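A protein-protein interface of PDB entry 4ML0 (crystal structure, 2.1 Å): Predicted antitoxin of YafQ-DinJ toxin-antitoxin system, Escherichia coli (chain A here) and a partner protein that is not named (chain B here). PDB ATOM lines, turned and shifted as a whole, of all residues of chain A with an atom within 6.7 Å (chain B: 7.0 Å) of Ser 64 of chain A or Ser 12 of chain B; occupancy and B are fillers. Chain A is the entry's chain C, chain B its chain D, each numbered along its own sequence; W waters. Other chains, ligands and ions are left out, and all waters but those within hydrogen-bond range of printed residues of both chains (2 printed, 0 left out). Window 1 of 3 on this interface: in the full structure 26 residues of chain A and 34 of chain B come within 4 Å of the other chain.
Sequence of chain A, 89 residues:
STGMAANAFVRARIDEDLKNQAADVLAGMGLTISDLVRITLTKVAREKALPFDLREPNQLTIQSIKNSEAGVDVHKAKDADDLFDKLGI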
ATOM      1  N   GLN A  59      15.831  27.074  36.179  1.00  0.00           N
ATOM      2  CA  GLN A  59      16.867  28.063  35.913  1.00  0.00           C
ATOM      3  C   GLN A  59      17.979  27.523  35.020  1.00  0.00           C
ATOM      4  O   GLN A  59      18.485  28.244  34.159  1.00  0.00           O
ATOM      5  CB  GLN A  59      17.437  28.622  37.225  1.00  0.00           C
ATOM      6  CG  GLN A  59      16.412  29.369  38.083  1.00  0.00           C
ATOM      7  CD  GLN A  59      15.696  28.469  39.094  1.00  0.00           C
ATOM      8  OE1 GLN A  59      15.485  27.264  38.859  1.00  0.00           O
ATOM      9  NE2 GLN A  59      15.318  29.057  40.232  1.00  0.00           N
ATOM     10  N   LEU A  60      18.355  26.260  35.214  1.00  0.00           N
ATOM     11  CA  LEU A  60      19.385  25.658  34.371  1.00  0.00           C
ATOM     12  C   LEU A  60      18.908  25.558  32.909  1.00  0.00           C
ATOM     13  O   LEU A  60      19.625  25.918  31.972  1.00  0.00           O
ATOM     14  CB  LEU A  60      19.816  24.279  34.911  1.00  0.00           C
ATOM     15  CG  LEU A  60      21.026  23.661  34.197  1.00  0.00           C
ATOM     16  CD1 LEU A  60      22.175  24.685  34.075  1.00  0.00           C
ATOM     17  CD2 LEU A  60      21.516  22.417  34.896  1.00  0.00           C
ATOM     18  N   THR A  61      17.688  25.083  32.719  1.00  0.00           N
ATOM     19  CA  THR A  61      17.168  24.926  31.365  1.00  0.00           C
ATOM     20  C   THR A  61      17.091  26.283  30.668  1.00  0.00           C
ATOM     21  O   THR A  61      17.486  26.426  29.497  1.00  0.00           O
ATOM     22  CB  THR A  61      15.792  24.247  31.384  1.00  0.00           C
ATOM     23  OG1 THR A  61      15.929  22.949  31.977  1.00  0.00           O
ATOM     24  CG2 THR A  61      15.253  24.088  29.971  1.00  0.00           C
ATOM     25  N   ILE A  62      16.597  27.276  31.399  1.00  0.00           N
ATOM     26  CA  ILE A  62      16.482  28.626  30.859  1.00  0.00           C
ATOM     27  C   ILE A  62      17.847  29.193  30.487  1.00  0.00           C
ATOM     28  O   ILE A  62      18.012  29.801  29.427  1.00  0.00           O
ATOM     29  CB  ILE A  62      15.783  29.576  31.849  1.00  0.00           C
ATOM     30  CG1 ILE A  62      14.293  29.242  31.949  1.00  0.00           C
ATOM     31  CG2 ILE A  62      15.971  31.041  31.425  1.00  0.00           C
ATOM     32  CD1 ILE A  62      13.507  29.531  30.665  1.00  0.00           C
ATOM     33  N   GLN A  63      18.831  28.998  31.359  1.00  0.00           N
ATOM     34  CA  GLN A  63      20.183  29.481  31.073  1.00  0.00           C
ATOM     35  C   GLN A  63      20.717  28.820  29.809  1.00  0.00           C
ATOM     36  O   GLN A  63      21.375  29.472  28.976  1.00  0.00           O
ATOM     37  CB  GLN A  63      21.124  29.199  32.254  1.00  0.00           C
ATOM     38  CG  GLN A  63      22.552  29.716  32.056  1.00  0.00           C
ATOM     39  CD  GLN A  63      22.628  31.239  31.981  1.00  0.00           C
ATOM     40  OE1 GLN A  63      22.189  31.948  32.895  1.00  0.00           O
ATOM     41  NE2 GLN A  63      23.185  31.748  30.885  1.00  0.00           N
ATOM     42  N   SER A  64      20.425  27.529  29.647  1.00  0.00           N
ATOM     43  CA  SER A  64      20.942  26.817  28.483  1.00  0.00           C
ATOM     44  C   SER A  64      20.307  27.355  27.208  1.00  0.00           C
ATOM     45  O   SER A  64      20.987  27.540  26.188  1.00  0.00           O
ATOM     46  CB  SER A  64      20.698  25.312  28.593  1.00  0.00           C
ATOM     47  OG  SER A  64      21.153  24.662  27.415  1.00  0.00           O
ATOM     48  N   ILE A  65      19.001  27.602  27.273  1.00  0.00           N
ATOM     49  CA  ILE A  65      18.273  28.152  26.138  1.00  0.00           C
ATOM     50  C   ILE A  65      18.785  29.547  25.770  1.00  0.00           C
ATOM     51  O   ILE A  65      19.021  29.820  24.593  1.00  0.00           O
ATOM     52  CB  ILE A  65      16.757  28.179  26.394  1.00  0.00           C
ATOM     53  CG1 ILE A  65      16.189  26.750  26.335  1.00  0.00           C
ATOM     54  CG2 ILE A  65      16.058  29.057  25.377  1.00  0.00           C
ATOM     55  CD1 ILE A  65      14.726  26.646  26.751  1.00  0.00           C
ATOM     56  N   LYS A  66      18.958  30.421  26.764  1.00  0.00           N
ATOM     57  CA  LYS A  66      19.539  31.757  26.526  1.00  0.00           C
ATOM     58  C   LYS A  66      20.927  31.697  25.883  1.00  0.00           C
ATOM     59  O   LYS A  66      21.194  32.394  24.906  1.00  0.00           O
ATOM     60  CB  LYS A  66      19.612  32.581  27.819  1.00  0.00           C
ATOM     61  CG  LYS A  66      18.263  33.106  28.326  1.00  0.00           C
ATOM     62  CD  LYS A  66      18.443  33.987  29.572  1.00  0.00           C
ATOM     63  CE  LYS A  66      17.094  34.376  30.182  1.00  0.00           C
ATOM     64  NZ  LYS A  66      17.247  35.007  31.541  1.00  0.00           N
ATOM     65  N   ASN A  67      21.815  30.878  26.438  1.00  0.00           N
ATOM     66  CA  ASN A  67      23.134  30.693  25.835  1.00  0.00           C
ATOM     67  C   ASN A  67      23.050  30.222  24.388  1.00  0.00           C
ATOM     68  O   ASN A  67      23.690  30.787  23.494  1.00  0.00           O
ATOM     69  CB  ASN A  67      23.971  29.693  26.637  1.00  0.00           C
ATOM     70  CG  ASN A  67      24.514  30.280  27.927  1.00  0.00           C
ATOM     71  OD1 ASN A  67      24.431  31.489  28.160  1.00  0.00           O
ATOM     72  ND2 ASN A  67      25.088  29.423  28.769  1.00  0.00           N
ATOM     73  N   SER A  68      22.271  29.170  24.165  1.00  0.00           N
ATOM     74  CA  SER A  68      22.101  28.621  22.830  1.00  0.00           C
ATOM     75  C   SER A  68      21.600  29.672  21.854  1.00  0.00           C
ATOM     76  O   SER A  68      22.118  29.797  20.739  1.00  0.00           O
ATOM     77  CB  SER A  68      21.157  27.419  22.852  1.00  0.00           C
ATOM     78  OG  SER A  68      21.828  26.286  23.365  1.00  0.00           O
ATOM     79  N   GLU A  69      20.606  30.434  22.291  1.00  0.00           N
ATOM     80  CA  GLU A  69      19.993  31.466  21.462  1.00  0.00           C
ATOM     81  C   GLU A  69      20.965  32.592  21.112  1.00  0.00           C
ATOM     82  O   GLU A  69      20.847  33.207  20.054  1.00  0.00           O
ATOM     83  CB  GLU A  69      18.750  32.037  22.152  1.00  0.00           C
ATOM     84  CG  GLU A  69      17.545  31.089  22.141  1.00  0.00           C
ATOM     85  CD  GLU A  69      17.084  30.721  20.732  1.00  0.00           C
ATOM     86  OE1 GLU A  69      16.857  29.517  20.467  1.00  0.00           O
ATOM     87  OE2 GLU A  69      16.944  31.634  19.887  1.00  0.00           O
ATOM     88  N   VAL A  72      26.104  30.912  22.225  1.00  0.00           N
ATOM     89  CA  VAL A  72      27.116  30.520  23.197  1.00  0.00           C
ATOM     90  C   VAL A  72      27.046  29.018  23.467  1.00  0.00           C
ATOM     91  O   VAL A  72      25.962  28.491  23.735  1.00  0.00           O
ATOM     92  CB  VAL A  72      26.889  31.251  24.540  1.00  0.00           C
ATOM     93  CG1 VAL A  72      27.903  30.777  25.589  1.00  0.00           C
ATOM     94  CG2 VAL A  72      26.944  32.774  24.353  1.00  0.00           C
ATOM     95  N   ASP A  73      28.193  28.337  23.406  1.00  0.00           N
ATOM     96  CA  ASP A  73      28.289  26.922  23.794  1.00  0.00           C
ATOM     97  C   ASP A  73      27.414  26.030  22.898  1.00  0.00           C
ATOM     98  O   ASP A  73      26.874  25.011  23.341  1.00  0.00           O
ATOM     99  CB  ASP A  73      27.900  26.757  25.270  1.00  0.00           C
ATOM    100  CG  ASP A  73      28.759  25.743  26.000  1.00  0.00           C
ATOM    101  OD1 ASP A  73      29.428  24.919  25.337  1.00  0.00           O
ATOM    102  OD2 ASP A  73      28.757  25.765  27.252  1.00  0.00           O
ATOM    103  N   VAL A  74      27.273  26.434  21.640  1.00  0.00           N
ATOM    104  CA  VAL A  74      26.522  25.676  20.644  1.00  0.00           C
ATOM    105  C   VAL A  74      27.506  24.938  19.738  1.00  0.00           C
ATOM    106  O   VAL A  74      28.487  25.522  19.281  1.00  0.00           O
ATOM    107  CB  VAL A  74      25.650  26.612  19.793  1.00  0.00           C
ATOM    108  CG1 VAL A  74      24.981  25.852  18.650  1.00  0.00           C
ATOM    109  CG2 VAL A  74      24.614  27.310  20.666  1.00  0.00           C
ATOM    110  N   HIS A  75      27.254  23.658  19.486  1.00  0.00           N
ATOM    111  CA  HIS A  75      28.173  22.863  18.680  1.00  0.00           C
ATOM    112  C   HIS A  75      27.446  22.232  17.498  1.00  0.00           C
ATOM    113  O   HIS A  75      26.244  21.963  17.575  1.00  0.00           O
ATOM    114  CB  HIS A  75      28.847  21.796  19.548  1.00  0.00           C
ATOM    115  CG  HIS A  75      29.388  22.330  20.839  1.00  0.00           C
ATOM    116  ND1 HIS A  75      30.551  23.070  20.910  1.00  0.00           N
ATOM    117  CD2 HIS A  75      28.915  22.250  22.108  1.00  0.00           C
ATOM    118  CE1 HIS A  75      30.774  23.418  22.167  1.00  0.00           C
ATOM    119  NE2 HIS A  75      29.797  22.933  22.913  1.00  0.00           N
ATOM    120  N   LEU A  87      29.316  13.173  21.247  1.00  0.00           N
ATOM    121  CA  LEU A  87      28.711  13.092  22.583  1.00  0.00           C
ATOM    122  C   LEU A  87      29.236  11.888  23.367  1.00  0.00           C
ATOM    123  O   LEU A  87      28.916  11.714  24.549  1.00  0.00           O
ATOM    124  CB  LEU A  87      27.181  13.011  22.495  1.00  0.00           C
ATOM    125  CG  LEU A  87      26.420  14.195  21.897  1.00  0.00           C
ATOM    126  CD1 LEU A  87      24.990  13.779  21.550  1.00  0.00           C
ATOM    127  CD2 LEU A  87      26.422  15.393  22.855  1.00  0.00           C
ATOM    128  N   GLU B  10      22.516  20.742  15.548  1.00  0.00           N
ATOM    129  CA  GLU B  10      23.296  21.311  16.651  1.00  0.00           C
ATOM    130  C   GLU B  10      23.028  20.580  17.966  1.00  0.00           C
ATOM    131  O   GLU B  10      22.038  19.844  18.102  1.00  0.00           O
ATOM    132  CB  GLU B  10      22.954  22.790  16.870  1.00  0.00           C
ATOM    133  CG  GLU B  10      23.240  23.720  15.721  1.00  0.00           C
ATOM    134  CD  GLU B  10      22.822  25.144  16.047  1.00  0.00           C
ATOM    135  OE1 GLU B  10      22.164  25.337  17.094  1.00  0.00           O
ATOM    136  OE2 GLU B  10      23.149  26.067  15.272  1.00  0.00           O
ATOM    137  N   TYR B  11      23.904  20.813  18.937  1.00  0.00           N
ATOM    138  CA  TYR B  11      23.646  20.436  20.321  1.00  0.00           C
ATOM    139  C   TYR B  11      24.314  21.468  21.220  1.00  0.00           C
ATOM    140  O   TYR B  11      25.336  22.053  20.845  1.00  0.00           O
ATOM    141  CB  TYR B  11      24.135  19.022  20.631  1.00  0.00           C
ATOM    142  CG  TYR B  11      25.635  18.827  20.534  1.00  0.00           C
ATOM    143  CD1 TYR B  11      26.232  18.489  19.327  1.00  0.00           C
ATOM    144  CD2 TYR B  11      26.447  18.958  21.656  1.00  0.00           C
ATOM    145  CE1 TYR B  11      27.597  18.297  19.234  1.00  0.00           C
ATOM    146  CE2 TYR B  11      27.811  18.768  21.576  1.00  0.00           C
ATOM    147  CZ  TYR B  11      28.382  18.438  20.362  1.00  0.00           C
ATOM    148  OH  TYR B  11      29.742  18.251  20.275  1.00  0.00           O
ATOM    149  N   SER B  12      23.723  21.711  22.390  1.00  0.00           N
ATOM    150  CA  SER B  12      24.257  22.693  23.335  1.00  0.00           C
ATOM    151  C   SER B  12      25.253  22.025  24.271  1.00  0.00           C
ATOM    152  O   SER B  12      25.187  20.805  24.488  1.00  0.00           O
ATOM    153  CB  SER B  12      23.122  23.276  24.167  1.00  0.00           C
ATOM    154  OG  SER B  12      22.648  22.294  25.066  1.00  0.00           O
ATOM    155  N   GLY B  13      26.159  22.815  24.852  1.00  0.00           N
ATOM    156  CA  GLY B  13      27.084  22.292  25.848  1.00  0.00           C
ATOM    157  C   GLY B  13      26.365  21.633  27.014  1.00  0.00           C
ATOM    158  O   GLY B  13      26.768  20.555  27.509  1.00  0.00           O
ATOM    159  N   GLN B  14      25.279  22.269  27.453  1.00  0.00           N
ATOM    160  CA  GLN B  14      24.498  21.688  28.529  1.00  0.00           C
ATOM    161  C   GLN B  14      24.011  20.305  28.120  1.00  0.00           C
ATOM    162  O   GLN B  14      23.984  19.392  28.943  1.00  0.00           O
ATOM    163  CB  GLN B  14      23.313  22.568  28.934  1.00  0.00           C
ATOM    164  CG  GLN B  14      22.690  22.097  30.242  1.00  0.00           C
ATOM    165  CD  GLN B  14      23.692  22.131  31.393  1.00  0.00           C
ATOM    166  OE1 GLN B  14      24.369  23.141  31.607  1.00  0.00           O
ATOM    167  NE2 GLN B  14      23.802  21.023  32.130  1.00  0.00           N
ATOM    168  N   PHE B  15      23.634  20.141  26.854  1.00  0.00           N
ATOM    169  CA  PHE B  15      23.201  18.821  26.385  1.00  0.00           C
ATOM    170  C   PHE B  15      24.300  17.764  26.523  1.00  0.00           C
ATOM    171  O   PHE B  15      24.035  16.652  26.976  1.00  0.00           O
ATOM    172  CB  PHE B  15      22.668  18.851  24.945  1.00  0.00           C
ATOM    173  CG  PHE B  15      22.102  17.518  24.486  1.00  0.00           C
ATOM    174  CD1 PHE B  15      20.890  17.048  24.991  1.00  0.00           C
ATOM    175  CD2 PHE B  15      22.780  16.739  23.553  1.00  0.00           C
ATOM    176  CE1 PHE B  15      20.364  15.807  24.578  1.00  0.00           C
ATOM    177  CE2 PHE B  15      22.262  15.513  23.130  1.00  0.00           C
ATOM    178  CZ  PHE B  15      21.047  15.043  23.649  1.00  0.00           C
ATOM    179  N   SER B  16      25.533  18.092  26.138  1.00  0.00           N
ATOM    180  CA  SER B  16      26.607  17.097  26.233  1.00  0.00           C
ATOM    181  C   SER B  16      26.825  16.713  27.694  1.00  0.00           C
ATOM    182  O   SER B  16      27.041  15.529  28.026  1.00  0.00           O
ATOM    183  CB  SER B  16      27.905  17.580  25.567  1.00  0.00           C
ATOM    184  OG  SER B  16      28.155  18.931  25.875  1.00  0.00           O
ATOM    185  N   LYS B  17      26.724  17.705  28.578  1.00  0.00           N
ATOM    186  CA  LYS B  17      26.785  17.414  30.013  1.00  0.00           C
ATOM    187  C   LYS B  17      25.630  16.524  30.517  1.00  0.00           C
ATOM    188  O   LYS B  17      25.841  15.602  31.328  1.00  0.00           O
ATOM    189  CB  LYS B  17      26.837  18.720  30.805  1.00  0.00           C
ATOM    190  CG  LYS B  17      28.097  19.556  30.540  1.00  0.00           C
ATOM    191  CD  LYS B  17      27.983  20.892  31.258  1.00  0.00           C
ATOM    192  CE  LYS B  17      29.339  21.497  31.595  1.00  0.00           C
ATOM    193  NZ  LYS B  17      29.176  22.661  32.544  1.00  0.00           N
ATOM    194  N   ASP B  18      24.413  16.794  30.048  1.00  0.00           N
ATOM    195  CA  ASP B  18      23.257  16.003  30.473  1.00  0.00           C
ATOM    196  C   ASP B  18      23.426  14.561  29.986  1.00  0.00           C
ATOM    197  O   ASP B  18      23.100  13.605  30.693  1.00  0.00           O
ATOM    198  CB  ASP B  18      21.950  16.595  29.927  1.00  0.00           C
ATOM    199  CG  ASP B  18      21.653  18.006  30.457  1.00  0.00           C
ATOM    200  OD1 ASP B  18      22.230  18.427  31.484  1.00  0.00           O
ATOM    201  OD2 ASP B  18      20.816  18.699  29.834  1.00  0.00           O
ATOM    202  N   TYR B  62      10.744  25.339  20.567  1.00  0.00           N
ATOM    203  CA  TYR B  62      11.218  24.314  21.494  1.00  0.00           C
ATOM    204  C   TYR B  62      10.157  23.257  21.764  1.00  0.00           C
ATOM    205  O   TYR B  62       8.972  23.566  21.944  1.00  0.00           O
ATOM    206  CB  TYR B  62      11.730  24.929  22.802  1.00  0.00           C
ATOM    207  CG  TYR B  62      13.114  25.524  22.667  1.00  0.00           C
ATOM    208  CD1 TYR B  62      14.248  24.737  22.830  1.00  0.00           C
ATOM    209  CD2 TYR B  62      13.288  26.872  22.366  1.00  0.00           C
ATOM    210  CE1 TYR B  62      15.515  25.275  22.698  1.00  0.00           C
ATOM    211  CE2 TYR B  62      14.550  27.424  22.234  1.00  0.00           C
ATOM    212  CZ  TYR B  62      15.657  26.622  22.398  1.00  0.00           C
ATOM    213  OH  TYR B  62      16.910  27.170  22.266  1.00  0.00           O
ATOM    214  N   ARG B  83      18.151  21.496  17.087  1.00  0.00           N
ATOM    215  CA  ARG B  83      19.152  21.623  18.162  1.00  0.00           C
ATOM    216  C   ARG B  83      18.794  20.797  19.391  1.00  0.00           C
ATOM    217  O   ARG B  83      17.743  21.005  19.999  1.00  0.00           O
ATOM    218  CB  ARG B  83      19.332  23.083  18.585  1.00  0.00           C
ATOM    219  CG  ARG B  83      20.397  23.269  19.698  1.00  0.00           C
ATOM    220  CD  ARG B  83      20.425  24.707  20.244  1.00  0.00           C
ATOM    221  NE  ARG B  83      20.477  25.695  19.172  1.00  0.00           N
ATOM    222  CZ  ARG B  83      19.749  26.802  19.129  1.00  0.00           C
ATOM    223  NH1 ARG B  83      18.901  27.084  20.112  1.00  0.00           N
ATOM    224  NH2 ARG B  83      19.876  27.631  18.099  1.00  0.00           N
ATOM    225  N   PHE B  84      19.661  19.864  19.766  1.00  0.00           N
ATOM    226  CA  PHE B  84      19.467  19.118  21.006  1.00  0.00           C
ATOM    227  C   PHE B  84      19.872  19.990  22.195  1.00  0.00           C
ATOM    228  O   PHE B  84      21.033  20.409  22.310  1.00  0.00           O
ATOM    229  CB  PHE B  84      20.234  17.787  20.964  1.00  0.00           C
ATOM    230  CG  PHE B  84      19.718  16.836  19.907  1.00  0.00           C
ATOM    231  CD1 PHE B  84      18.498  16.184  20.077  1.00  0.00           C
ATOM    232  CD2 PHE B  84      20.436  16.619  18.731  1.00  0.00           C
ATOM    233  CE1 PHE B  84      18.004  15.317  19.099  1.00  0.00           C
ATOM    234  CE2 PHE B  84      19.957  15.751  17.749  1.00  0.00           C
ATOM    235  CZ  PHE B  84      18.732  15.099  17.934  1.00  0.00           C
ATOM    236  N   GLU B  85      18.916  20.277  23.078  1.00  0.00           N
ATOM    237  CA  GLU B  85      19.125  21.327  24.076  1.00  0.00           C
ATOM    238  C   GLU B  85      19.431  20.847  25.498  1.00  0.00           C
ATOM    239  O   GLU B  85      20.405  21.296  26.097  1.00  0.00           O
ATOM    240  CB  GLU B  85      17.939  22.296  24.092  1.00  0.00           C
ATOM    241  CG  GLU B  85      18.204  23.559  24.891  1.00  0.00           C
ATOM    242  CD  GLU B  85      19.206  24.488  24.210  1.00  0.00           C
ATOM    243  OE1 GLU B  85      19.046  24.754  23.005  1.00  0.00           O
ATOM    244  OE2 GLU B  85      20.146  24.959  24.888  1.00  0.00           O
ATOM    245  N   ARG B  86      18.578  19.982  26.049  1.00  0.00           N
ATOM    246  CA  ARG B  86      18.809  19.399  27.366  1.00  0.00           C
ATOM    247  C   ARG B  86      18.213  18.010  27.406  1.00  0.00           C
ATOM    248  O   ARG B  86      17.423  17.657  26.539  1.00  0.00           O
ATOM    249  CB  ARG B  86      18.181  20.252  28.482  1.00  0.00           C
ATOM    250  CG  ARG B  86      18.950  21.539  28.790  1.00  0.00           C
ATOM    251  CD  ARG B  86      18.898  21.860  30.260  1.00  0.00           C
ATOM    252  NE  ARG B  86      19.496  20.803  31.076  1.00  0.00           N
ATOM    253  CZ  ARG B  86      19.216  20.618  32.361  1.00  0.00           C
ATOM    254  NH1 ARG B  86      18.340  21.411  32.957  1.00  0.00           N
ATOM    255  NH2 ARG B  86      19.793  19.637  33.044  1.00  0.00           N
HETATM  256  O   HOH W   1      18.159  29.326  17.563  1.00  0.00           O
HETATM  257  O   HOH W   2      24.063  24.979  26.889  1.00  0.00           O
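The side-chain hydroxyl (OG1) of Thr 61 of chain A lies within hydrogen-bond range of the guanidinium group (NH1) of Arg 86 of chain B, at 3.0 Å. OG of Ser 64 of chain A lies within hydrogen-bond range of OE2 of Glu 85 of chain B. OG of Ser 68 of chain A lies within hydrogen-bond range of OE2 of Glu 85 of chain B. OE1 of Glu 69 of chain A sits at hydrogen-bond distance from OH of Tyr 62 of chain B (3.0 Å). The guanidinium group of Arg 83 of chain B is in salt-bridge range of the side-chain carboxylate of Glu 69 of chain A. O of Asp 73 of chain A sits at hydrogen-bond distance from N of Gly 13 of chain B, at 2.8 Å. The backbone carbonyl oxygen of Tyr 11 of chain B sits at hydrogen-bond distance from the backbone NH of His 75 of chain A (2.8 Å).
The backbone carbonyl oxygen (O) of Ser 64 of chain A lies within hydrogen-bond range of the side-chain hydroxyl (OG) of Ser 68 of chain A (3.2 Å). The side-chain carboxylate (OE1) of Glu 10 of chain B lies within salt-bridge range of the guanidinium group (NE) of Arg 83 of chain B (2.7 Å). O of Phe 84 of chain B sits at hydrogen-bond distance from N of Ser 12 of chain B (3.0 Å). The side-chain amide nitrogen of Gln 14 of chain B sits at hydrogen-bond distance from the side-chain carboxylate of Asp 18 of chain B (3.1 Å). OH of Tyr 62 of chain B lies within hydrogen-bond range of NH1 of Arg 83 of chain B, at 2.9 Å. The side-chain hydroxyl (OH) of Tyr 62 of chain B sits at hydrogen-bond distance from the side-chain carboxylate (OE1) of Glu 85 of chain B (3.3 Å).
Leu 60 of chain A touches Gln 14 of chain B (CD1 to OE1, 3.6 Å). Ser 64 of chain A touches Gln 14 of chain B (OG to CB, 3.4 Å). Ile 65 of chain A touches Tyr 62 of chain B (CG2 to OH, 3.7 Å). OE2 of Glu 85 of chain B touches N of Ile 65 of chain A, at 3.7 Å. Ser 68 of chain A touches Arg 83 of chain B (CB to NH1, 3.6 Å). Val 74 of chain A touches Glu 10 of chain B. His 75 of chain A touches Glu 10 of chain B (O to CA, 3.2 Å). His 75 of chain A touches Gly 13 of chain B. Leu 87 of chain A touches Tyr 11 of chain B. Ser 16 of chain B touches Leu 87 of chain A.
Printed residues of chain B within 4 Å of Ser 64 of chain A: Ser 12 (3.7 Å), Gln 14 (3.4 Å) and Glu 85 (2.7 Å). Of the printed residues of chain B, Glu 69 of chain A touches Tyr 62 and Arg 83. Of the printed residues of chain B, His 75 of chain A touches Glu 10, Tyr 11 and Gly 13. Printed residues of chain A within 4 Å of Glu 10 of chain B: Val 74 (3.3 Å) and His 75 (3.2 Å). Of chain A, only Ser 64, Ser 68 and Asp 73 come within 4 Å of Ser 12 of chain B. Asp 18 of chain B touches none of the printed residues of chain A. Of the printed residues of chain A, Glu 85 of chain B touches Ser 64 (2.7 Å), Ile 65 (3.7 Å) and Ser 68 (2.6 Å). Printed residues of chain A within 4 Å of Arg 86 of chain B: Leu 60 (3.7 Å) and Thr 61 (3.0 Å). The nearest residue of chain B that does not touch Ser 64 of chain A is Arg 86 of chain B (4.1 Å). The nearest residue of chain A that does not touch Ser 12 of chain B is His 75 of chain A (4.3 Å). The nearest printed residue of chain A that does not touch Arg 83 of chain B is Val 74 of chain A (4.5 Å).
Of the 14 printed residues of chain B, 11 touch a printed residue of chain A. Hydrophobic or aromatic side chains of chain B that line the printed part of chain A: Tyr 11, Phe 15 and Tyr 62. Along chain B the printed residues that touch a printed residue of chain A span positions 10 to 86. Hydrophobic or aromatic side chains of chain A that line the printed part of chain B: Leu 60, Ile 65, Val 74, His 75 and Leu 87.
Water W1 bridges NH2 of Arg 83 of chain B (2.5 Å) and OE1 of Glu 69 of chain A (3.2 Å). Water W2 lies within hydrogen-bond range of OG of Ser 64 of chain A (3.0 Å) and N of Gln 14 of chain B (3.0 Å).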
